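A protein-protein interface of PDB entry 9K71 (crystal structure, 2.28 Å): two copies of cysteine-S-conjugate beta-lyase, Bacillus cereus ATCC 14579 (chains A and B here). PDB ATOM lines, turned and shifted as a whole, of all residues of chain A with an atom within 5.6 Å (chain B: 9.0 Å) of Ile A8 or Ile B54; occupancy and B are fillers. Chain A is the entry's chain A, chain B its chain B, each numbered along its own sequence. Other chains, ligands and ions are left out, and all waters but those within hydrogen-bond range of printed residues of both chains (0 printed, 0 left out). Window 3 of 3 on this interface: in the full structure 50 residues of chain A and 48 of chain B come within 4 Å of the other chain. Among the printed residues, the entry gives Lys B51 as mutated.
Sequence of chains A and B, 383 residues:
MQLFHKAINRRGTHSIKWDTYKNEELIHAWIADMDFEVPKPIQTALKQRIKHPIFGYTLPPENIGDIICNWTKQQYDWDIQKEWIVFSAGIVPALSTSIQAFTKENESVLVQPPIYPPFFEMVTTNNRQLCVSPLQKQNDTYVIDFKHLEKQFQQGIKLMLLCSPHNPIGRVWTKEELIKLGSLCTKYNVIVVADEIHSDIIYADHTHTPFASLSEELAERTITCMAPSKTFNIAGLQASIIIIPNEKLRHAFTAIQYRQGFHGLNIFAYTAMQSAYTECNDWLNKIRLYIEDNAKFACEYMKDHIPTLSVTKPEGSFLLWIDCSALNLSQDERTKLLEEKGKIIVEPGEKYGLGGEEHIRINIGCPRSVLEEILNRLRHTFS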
ATOM      1  N   LYS A   6      34.338 -17.747 -18.094  1.00  0.00           N
ATOM      2  CA  LYS A   6      34.516 -19.149 -18.522  1.00  0.00           C
ATOM      3  C   LYS A   6      33.974 -19.547 -19.877  1.00  0.00           C
ATOM      4  O   LYS A   6      32.771 -19.828 -19.931  1.00  0.00           O
ATOM      5  CB  LYS A   6      33.683 -19.991 -17.558  1.00  0.00           C
ATOM      6  CG  LYS A   6      34.460 -20.847 -16.570  1.00  0.00           C
ATOM      7  CD  LYS A   6      33.558 -21.746 -15.758  1.00  0.00           C
ATOM      8  CE  LYS A   6      34.252 -22.337 -14.550  1.00  0.00           C
ATOM      9  NZ  LYS A   6      33.291 -22.982 -13.625  1.00  0.00           N
ATOM     10  N   ALA A   7      34.818 -19.612 -20.913  1.00  0.00           N
ATOM     11  CA  ALA A   7      34.337 -20.275 -22.096  1.00  0.00           C
ATOM     12  C   ALA A   7      34.301 -21.788 -21.836  1.00  0.00           C
ATOM     13  O   ALA A   7      35.319 -22.397 -21.471  1.00  0.00           O
ATOM     14  CB  ALA A   7      35.233 -19.917 -23.292  1.00  0.00           C
ATOM     15  N   ILE A   8      33.134 -22.410 -22.040  1.00  0.00           N
ATOM     16  CA  ILE A   8      32.925 -23.819 -21.688  1.00  0.00           C
ATOM     17  C   ILE A   8      32.598 -24.625 -22.940  1.00  0.00           C
ATOM     18  O   ILE A   8      31.745 -24.227 -23.745  1.00  0.00           O
ATOM     19  CB  ILE A   8      31.826 -24.017 -20.628  1.00  0.00           C
ATOM     20  CG1 ILE A   8      31.906 -22.979 -19.519  1.00  0.00           C
ATOM     21  CG2 ILE A   8      31.898 -25.404 -20.044  1.00  0.00           C
ATOM     22  CD1 ILE A   8      30.530 -22.592 -19.039  1.00  0.00           C
ATOM     23  N   ASN A   9      33.281 -25.752 -23.091  1.00  0.00           N
ATOM     24  CA  ASN A   9      33.014 -26.743 -24.122  1.00  0.00           C
ATOM     25  C   ASN A   9      31.677 -27.426 -23.843  1.00  0.00           C
ATOM     26  O   ASN A   9      31.584 -28.319 -22.998  1.00  0.00           O
ATOM     27  CB  ASN A   9      34.153 -27.753 -24.137  1.00  0.00           C
ATOM     28  CG  ASN A   9      33.965 -28.813 -25.171  1.00  0.00           C
ATOM     29  OD1 ASN A   9      33.409 -28.553 -26.233  1.00  0.00           O
ATOM     30  ND2 ASN A   9      34.414 -30.033 -24.869  1.00  0.00           N
ATOM     31  N   ARG A  10      30.638 -27.032 -24.582  1.00  0.00           N
ATOM     32  CA  ARG A  10      29.325 -27.648 -24.452  1.00  0.00           C
ATOM     33  C   ARG A  10      28.996 -28.514 -25.657  1.00  0.00           C
ATOM     34  O   ARG A  10      27.833 -28.896 -25.847  1.00  0.00           O
ATOM     35  CB  ARG A  10      28.231 -26.592 -24.285  1.00  0.00           C
ATOM     36  CG  ARG A  10      28.293 -25.769 -23.017  1.00  0.00           C
ATOM     37  CD  ARG A  10      27.017 -24.928 -22.833  1.00  0.00           C
ATOM     38  NE  ARG A  10      25.807 -25.740 -22.700  1.00  0.00           N
ATOM     39  CZ  ARG A  10      24.568 -25.250 -22.722  1.00  0.00           C
ATOM     40  NH1 ARG A  10      24.373 -23.945 -22.881  1.00  0.00           N
ATOM     41  NH2 ARG A  10      23.521 -26.065 -22.587  1.00  0.00           N
ATOM     42  N   ARG A  11      30.008 -28.842 -26.455  1.00  0.00           N
ATOM     43  CA  ARG A  11      29.902 -29.837 -27.508  1.00  0.00           C
ATOM     44  C   ARG A  11      30.049 -31.218 -26.894  1.00  0.00           C
ATOM     45  O   ARG A  11      30.929 -31.441 -26.058  1.00  0.00           O
ATOM     46  CB  ARG A  11      30.994 -29.626 -28.562  1.00  0.00           C
ATOM     47  CG  ARG A  11      31.034 -28.238 -29.198  1.00  0.00           C
ATOM     48  CD  ARG A  11      32.165 -27.375 -28.654  1.00  0.00           C
ATOM     49  NE  ARG A  11      32.037 -25.990 -29.093  1.00  0.00           N
ATOM     50  CZ  ARG A  11      31.088 -25.162 -28.664  1.00  0.00           C
ATOM     51  NH1 ARG A  11      30.186 -25.577 -27.778  1.00  0.00           N
ATOM     52  NH2 ARG A  11      31.045 -23.917 -29.117  1.00  0.00           N
ATOM     53  N   ASP A  33      19.319 -21.097 -23.680  1.00  0.00           N
ATOM     54  CA  ASP A  33      20.001 -21.417 -22.430  1.00  0.00           C
ATOM     55  C   ASP A  33      21.337 -20.674 -22.381  1.00  0.00           C
ATOM     56  O   ASP A  33      21.865 -20.259 -23.406  1.00  0.00           O
ATOM     57  CB  ASP A  33      20.154 -22.944 -22.218  1.00  0.00           C
ATOM     58  CG  ASP A  33      21.151 -23.627 -23.187  1.00  0.00           C
ATOM     59  OD1 ASP A  33      21.965 -22.960 -23.858  1.00  0.00           O
ATOM     60  OD2 ASP A  33      21.130 -24.878 -23.255  1.00  0.00           O
ATOM     61  N   MET A  34      21.891 -20.525 -21.182  1.00  0.00           N
ATOM     62  CA  MET A  34      23.101 -19.733 -21.006  1.00  0.00           C
ATOM     63  C   MET A  34      24.354 -20.532 -21.350  1.00  0.00           C
ATOM     64  O   MET A  34      24.333 -21.762 -21.433  1.00  0.00           O
ATOM     65  CB  MET A  34      23.217 -19.226 -19.565  1.00  0.00           C
ATOM     66  CG  MET A  34      21.971 -18.549 -19.040  1.00  0.00           C
ATOM     67  SD  MET A  34      22.156 -17.791 -17.399  1.00  0.00           S
ATOM     68  CE  MET A  34      22.885 -19.122 -16.450  1.00  0.00           C
ATOM     69  N   ASP A  35      25.444 -19.798 -21.612  1.00  0.00           N
ATOM     70  CA  ASP A  35      26.800 -20.347 -21.727  1.00  0.00           C
ATOM     71  C   ASP A  35      27.524 -20.249 -20.402  1.00  0.00           C
ATOM     72  O   ASP A  35      28.676 -19.788 -20.321  1.00  0.00           O
ATOM     73  CB  ASP A  35      27.593 -19.628 -22.816  1.00  0.00           C
ATOM     74  CG  ASP A  35      27.492 -20.303 -24.159  1.00  0.00           C
ATOM     75  OD1 ASP A  35      26.816 -21.353 -24.261  1.00  0.00           O
ATOM     76  OD2 ASP A  35      28.090 -19.777 -25.118  1.00  0.00           O
ATOM     77  N   PHE A  36      26.804 -20.548 -19.330  1.00  0.00           N
ATOM     78  CA  PHE A  36      27.324 -20.420 -17.980  1.00  0.00           C
ATOM     79  C   PHE A  36      27.073 -21.682 -17.191  1.00  0.00           C
ATOM     80  O   PHE A  36      26.034 -22.331 -17.368  1.00  0.00           O
ATOM     81  CB  PHE A  36      26.687 -19.251 -17.294  1.00  0.00           C
ATOM     82  CG  PHE A  36      27.046 -17.953 -17.918  1.00  0.00           C
ATOM     83  CD1 PHE A  36      28.360 -17.676 -18.209  1.00  0.00           C
ATOM     84  CD2 PHE A  36      26.066 -17.013 -18.213  1.00  0.00           C
ATOM     85  CE1 PHE A  36      28.695 -16.483 -18.801  1.00  0.00           C
ATOM     86  CE2 PHE A  36      26.396 -15.795 -18.782  1.00  0.00           C
ATOM     87  CZ  PHE A  36      27.710 -15.529 -19.078  1.00  0.00           C
ATOM     88  N   VAL A  38      26.039 -23.946 -14.075  1.00  0.00           N
ATOM     89  CA  VAL A  38      25.183 -23.947 -12.905  1.00  0.00           C
ATOM     90  C   VAL A  38      26.048 -23.521 -11.727  1.00  0.00           C
ATOM     91  O   VAL A  38      27.194 -23.985 -11.607  1.00  0.00           O
ATOM     92  CB  VAL A  38      24.563 -25.331 -12.694  1.00  0.00           C
ATOM     93  CG1 VAL A  38      23.355 -25.220 -11.860  1.00  0.00           C
ATOM     94  CG2 VAL A  38      24.182 -25.929 -14.025  1.00  0.00           C
ATOM     95  N   ASN A 233      19.984 -22.025 -15.429  1.00  0.00           N
ATOM     96  CA  ASN A 233      20.530 -22.833 -16.515  1.00  0.00           C
ATOM     97  C   ASN A 233      20.343 -24.331 -16.267  1.00  0.00           C
ATOM     98  O   ASN A 233      21.193 -25.149 -16.611  1.00  0.00           O
ATOM     99  CB  ASN A 233      22.002 -22.492 -16.723  1.00  0.00           C
ATOM    100  CG  ASN A 233      22.488 -22.829 -18.105  1.00  0.00           C
ATOM    101  OD1 ASN A 233      21.705 -22.906 -19.044  1.00  0.00           O
ATOM    102  ND2 ASN A 233      23.798 -23.029 -18.241  1.00  0.00           N
ATOM    103  N   PRO A 367      29.964 -15.823 -21.973  1.00  0.00           N
ATOM    104  CA  PRO A 367      31.201 -15.099 -21.677  1.00  0.00           C
ATOM    105  C   PRO A 367      31.432 -13.984 -22.680  1.00  0.00           C
ATOM    106  O   PRO A 367      31.143 -14.125 -23.872  1.00  0.00           O
ATOM    107  CB  PRO A 367      32.267 -16.191 -21.785  1.00  0.00           C
ATOM    108  CG  PRO A 367      31.503 -17.412 -21.377  1.00  0.00           C
ATOM    109  CD  PRO A 367      30.118 -17.281 -21.858  1.00  0.00           C
ATOM    110  N   ARG B  49      27.843 -37.650 -15.747  1.00  0.00           N
ATOM    111  CA  ARG B  49      27.301 -36.506 -16.472  1.00  0.00           C
ATOM    112  C   ARG B  49      27.261 -35.238 -15.610  1.00  0.00           C
ATOM    113  O   ARG B  49      27.399 -34.130 -16.143  1.00  0.00           O
ATOM    114  CB  ARG B  49      25.923 -36.831 -17.049  1.00  0.00           C
ATOM    115  CG  ARG B  49      25.581 -35.921 -18.240  1.00  0.00           C
ATOM    116  CD  ARG B  49      24.359 -35.116 -17.922  1.00  0.00           C
ATOM    117  NE  ARG B  49      24.083 -34.015 -18.845  1.00  0.00           N
ATOM    118  CZ  ARG B  49      24.684 -32.831 -18.825  1.00  0.00           C
ATOM    119  NH1 ARG B  49      25.622 -32.576 -17.926  1.00  0.00           N
ATOM    120  NH2 ARG B  49      24.312 -31.890 -19.682  1.00  0.00           N
ATOM    121  N   ILE B  50      27.067 -35.378 -14.293  1.00  0.00           N
ATOM    122  CA  ILE B  50      27.060 -34.241 -13.371  1.00  0.00           C
ATOM    123  C   ILE B  50      28.401 -33.522 -13.352  1.00  0.00           C
ATOM    124  O   ILE B  50      28.470 -32.342 -12.992  1.00  0.00           O
ATOM    125  CB  ILE B  50      26.663 -34.745 -11.965  1.00  0.00           C
ATOM    126  CG1 ILE B  50      25.151 -34.700 -11.787  1.00  0.00           C
ATOM    127  CG2 ILE B  50      27.345 -34.000 -10.842  1.00  0.00           C
ATOM    128  CD1 ILE B  50      24.715 -35.373 -10.519  1.00  0.00           C
ATOM    129  N   LYS B  51      29.467 -34.197 -13.780  1.00  0.00           N
ATOM    130  CA  LYS B  51      30.801 -33.541 -13.874  1.00  0.00           C
ATOM    131  C   LYS B  51      30.773 -32.406 -14.909  1.00  0.00           C
ATOM    132  O   LYS B  51      31.596 -31.505 -14.794  1.00  0.00           O
ATOM    133  CB  LYS B  51      31.907 -34.572 -14.102  1.00  0.00           C
ATOM    134  CG  LYS B  51      32.567 -35.103 -12.843  1.00  0.00           C
ATOM    135  CD  LYS B  51      33.198 -36.449 -13.061  1.00  0.00           C
ATOM    136  CE  LYS B  51      33.078 -37.355 -11.859  1.00  0.00           C
ATOM    137  NZ  LYS B  51      33.996 -38.510 -11.968  1.00  0.00           N
ATOM    138  N   HIS B  52      29.827 -32.427 -15.840  1.00  0.00           N
ATOM    139  CA  HIS B  52      29.711 -31.335 -16.796  1.00  0.00           C
ATOM    140  C   HIS B  52      28.683 -30.346 -16.266  1.00  0.00           C
ATOM    141  O   HIS B  52      27.477 -30.504 -16.505  1.00  0.00           O
ATOM    142  CB  HIS B  52      29.317 -31.838 -18.188  1.00  0.00           C
ATOM    143  CG  HIS B  52      29.121 -30.738 -19.182  1.00  0.00           C
ATOM    144  ND1 HIS B  52      30.172 -30.047 -19.746  1.00  0.00           N
ATOM    145  CD2 HIS B  52      27.994 -30.179 -19.680  1.00  0.00           C
ATOM    146  CE1 HIS B  52      29.703 -29.119 -20.561  1.00  0.00           C
ATOM    147  NE2 HIS B  52      28.383 -29.179 -20.540  1.00  0.00           N
ATOM    148  N   PRO B  53      29.109 -29.306 -15.646  1.00  0.00           N
ATOM    149  CA  PRO B  53      28.217 -28.487 -14.829  1.00  0.00           C
ATOM    150  C   PRO B  53      27.298 -27.547 -15.582  1.00  0.00           C
ATOM    151  O   PRO B  53      27.149 -26.381 -15.200  1.00  0.00           O
ATOM    152  CB  PRO B  53      29.200 -27.715 -13.946  1.00  0.00           C
ATOM    153  CG  PRO B  53      30.445 -27.786 -14.651  1.00  0.00           C
ATOM    154  CD  PRO B  53      30.517 -28.995 -15.416  1.00  0.00           C
ATOM    155  N   ILE B  54      26.654 -28.041 -16.633  1.00  0.00           N
ATOM    156  CA  ILE B  54      25.554 -27.313 -17.256  1.00  0.00           C
ATOM    157  C   ILE B  54      24.461 -28.313 -17.589  1.00  0.00           C
ATOM    158  O   ILE B  54      24.739 -29.456 -17.974  1.00  0.00           O
ATOM    159  CB  ILE B  54      26.006 -26.517 -18.495  1.00  0.00           C
ATOM    160  CG1 ILE B  54      26.931 -25.375 -18.079  1.00  0.00           C
ATOM    161  CG2 ILE B  54      24.817 -25.927 -19.220  1.00  0.00           C
ATOM    162  CD1 ILE B  54      27.878 -24.924 -19.175  1.00  0.00           C
ATOM    163  N   PHE B  55      23.217 -27.893 -17.398  1.00  0.00           N
ATOM    164  CA  PHE B  55      22.085 -28.800 -17.453  1.00  0.00           C
ATOM    165  C   PHE B  55      20.952 -28.180 -18.256  1.00  0.00           C
ATOM    166  O   PHE B  55      19.793 -28.181 -17.840  1.00  0.00           O
ATOM    167  CB  PHE B  55      21.641 -29.161 -16.042  1.00  0.00           C
ATOM    168  CG  PHE B  55      22.704 -29.848 -15.233  1.00  0.00           C
ATOM    169  CD1 PHE B  55      23.226 -31.067 -15.642  1.00  0.00           C
ATOM    170  CD2 PHE B  55      23.188 -29.271 -14.064  1.00  0.00           C
ATOM    171  CE1 PHE B  55      24.209 -31.703 -14.894  1.00  0.00           C
ATOM    172  CE2 PHE B  55      24.179 -29.895 -13.316  1.00  0.00           C
ATOM    173  CZ  PHE B  55      24.690 -31.110 -13.733  1.00  0.00           C
ATOM    174  N   GLY B  56      21.279 -27.647 -19.435  1.00  0.00           N
ATOM    175  CA  GLY B  56      20.275 -27.062 -20.297  1.00  0.00           C
ATOM    176  C   GLY B  56      19.454 -28.120 -21.018  1.00  0.00           C
ATOM    177  O   GLY B  56      19.472 -29.307 -20.680  1.00  0.00           O
ATOM    178  N   TYR B  57      18.728 -27.672 -22.036  1.00  0.00           N
ATOM    179  CA  TYR B  57      17.936 -28.597 -22.832  1.00  0.00           C
ATOM    180  C   TYR B  57      18.868 -29.561 -23.544  1.00  0.00           C
ATOM    181  O   TYR B  57      19.862 -29.150 -24.147  1.00  0.00           O
ATOM    182  CB  TYR B  57      17.107 -27.851 -23.871  1.00  0.00           C
ATOM    183  CG  TYR B  57      16.272 -26.672 -23.406  1.00  0.00           C
ATOM    184  CD1 TYR B  57      16.784 -25.365 -23.436  1.00  0.00           C
ATOM    185  CD2 TYR B  57      14.949 -26.851 -23.009  1.00  0.00           C
ATOM    186  CE1 TYR B  57      16.008 -24.281 -23.056  1.00  0.00           C
ATOM    187  CE2 TYR B  57      14.172 -25.784 -22.621  1.00  0.00           C
ATOM    188  CZ  TYR B  57      14.705 -24.491 -22.649  1.00  0.00           C
ATOM    189  OH  TYR B  57      13.922 -23.424 -22.258  1.00  0.00           O
ATOM    190  N   THR B  58      18.567 -30.849 -23.475  1.00  0.00           N
ATOM    191  CA  THR B  58      19.417 -31.792 -24.171  1.00  0.00           C
ATOM    192  C   THR B  58      18.575 -32.706 -25.033  1.00  0.00           C
ATOM    193  O   THR B  58      17.459 -33.087 -24.662  1.00  0.00           O
ATOM    194  CB  THR B  58      20.323 -32.598 -23.212  1.00  0.00           C
ATOM    195  OG1 THR B  58      19.574 -33.606 -22.521  1.00  0.00           O
ATOM    196  CG2 THR B  58      21.061 -31.653 -22.235  1.00  0.00           C
ATOM    197  N   ILE B 267      17.335 -34.633 -18.563  1.00  0.00           N
ATOM    198  CA  ILE B 267      18.716 -35.006 -18.860  1.00  0.00           C
ATOM    199  C   ILE B 267      19.065 -36.356 -18.237  1.00  0.00           C
ATOM    200  O   ILE B 267      19.740 -37.189 -18.854  1.00  0.00           O
ATOM    201  CB  ILE B 267      19.658 -33.891 -18.366  1.00  0.00           C
ATOM    202  CG1 ILE B 267      19.568 -32.658 -19.241  1.00  0.00           C
ATOM    203  CG2 ILE B 267      21.070 -34.320 -18.360  1.00  0.00           C
ATOM    204  CD1 ILE B 267      20.417 -31.570 -18.704  1.00  0.00           C
ATOM    205  N   PHE B 268      18.599 -36.595 -17.013  1.00  0.00           N
ATOM    206  CA  PHE B 268      18.982 -37.763 -16.225  1.00  0.00           C
ATOM    207  C   PHE B 268      18.125 -38.983 -16.508  1.00  0.00           C
ATOM    208  O   PHE B 268      18.510 -40.100 -16.136  1.00  0.00           O
ATOM    209  CB  PHE B 268      18.925 -37.423 -14.734  1.00  0.00           C
ATOM    210  CG  PHE B 268      19.972 -36.430 -14.299  1.00  0.00           C
ATOM    211  CD1 PHE B 268      21.310 -36.785 -14.278  1.00  0.00           C
ATOM    212  CD2 PHE B 268      19.619 -35.145 -13.924  1.00  0.00           C
ATOM    213  CE1 PHE B 268      22.276 -35.881 -13.872  1.00  0.00           C
ATOM    214  CE2 PHE B 268      20.571 -34.245 -13.516  1.00  0.00           C
ATOM    215  CZ  PHE B 268      21.905 -34.610 -13.491  1.00  0.00           C
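No position is printed for both chains.
Of the 12 pairs that touch across the chains among the printed residues, none has its exchanged pair printed and touching as well.
Among the printed residues, pairs that only touch across the chains: Asn A9 with His B52 (3.2 Å), Asn A233 with Ile B54 (3.2 Å), Phe A36 with Ile B54 (3.3 Å), Val A38 with Phe B55 (3.5 Å), Ile A8 with Ile B54 (3.5 Å), Arg A10 with Ile B54 (3.6 Å), Asn A233 with Gly B56 (3.8 Å), Val A38 with Ile B54 (3.8 Å), Asp A33 with Gly B56 (3.8 Å) and Asp A33 with Tyr B57 (3.9 Å).
Of chain B, only Ile B54 comes within 4 Å of Ile A8.
Of chain A, only Ile A8, Arg A10, Phe A36, Val A38 and Asn A233 come within 4 Å of Ile B54.
Of the printed residues of chain B, Asp A33 touches Gly B56 and Tyr B57.
Printed residues of chain A within 4 Å of Tyr B57: Asp A33 (3.9 Å).
Printed residues of chain B within 4 Å of Val A38: Pro B53 (2.9 Å), Ile B54 (3.8 Å) and Phe B55 (3.5 Å).
Printed residues of chain B within 4 Å of Asn A9: His B52 (3.2 Å).
The nearest residue of chain A that does not touch Ile B54 is Met A34 (4.7 Å).
The nearest printed residue of chain B that does not touch Asp A33 is Ile B54 (5.6 Å).
The backbone NH (N) of Val A38 is in hydrogen-bond range of the backbone carbonyl oxygen (O) of Pro B53, at 2.9 Å.
The backbone NH (N) of Phe B55 lies close to the backbone carbonyl oxygen (O) of Asn A233.
O of Met A34 lies within hydrogen-bond range of NH1 of Arg A10, 2.6 Å away.
The side-chain amide oxygen (OD1) of Asn A9 sits close to the backbone NH (N) of Arg A11, at 3.4 Å.
ND2 of Asn A233 sits at hydrogen-bond distance from O of Phe A36 (2.5 Å).
The guanidinium group (NH2) of Arg B49 lies within hydrogen-bond range of the backbone carbonyl oxygen (O) of Ile B54 (3.0 Å).
The side-chain carboxylate (OD1) of Asp A35 lies within salt-bridge range of the guanidinium group (NH1) of Arg A10.
The backbone carbonyl oxygen of His B52 is in hydrogen-bond range of the guanidinium group of Arg B49 (3.1 Å).
Of the 13 printed residues of chain A, 7 touch a printed residue of chain B.
Printed residues of chain A that touch a printed residue of chain B: Ile A8, Asn A9, Arg A10, Asp A33, Phe A36, Val A38 and Asn A233.
Printed residues of chain B that touch a printed residue of chain A: His B52, Pro B53, Ile B54, Phe B55, Gly B56 and Tyr B57.
Hydrophobic or aromatic side chains of chain B within 4 Å of the printed part of chain A: His B52, Ile B54 and Phe B55.
Along chain B the printed residues that touch a printed residue of chain A span positions 52 to 57.
Among the printed residues, no Asp or Glu carboxylate lies within 4 Å of a Lys or Arg side-chain nitrogen of the other chain.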
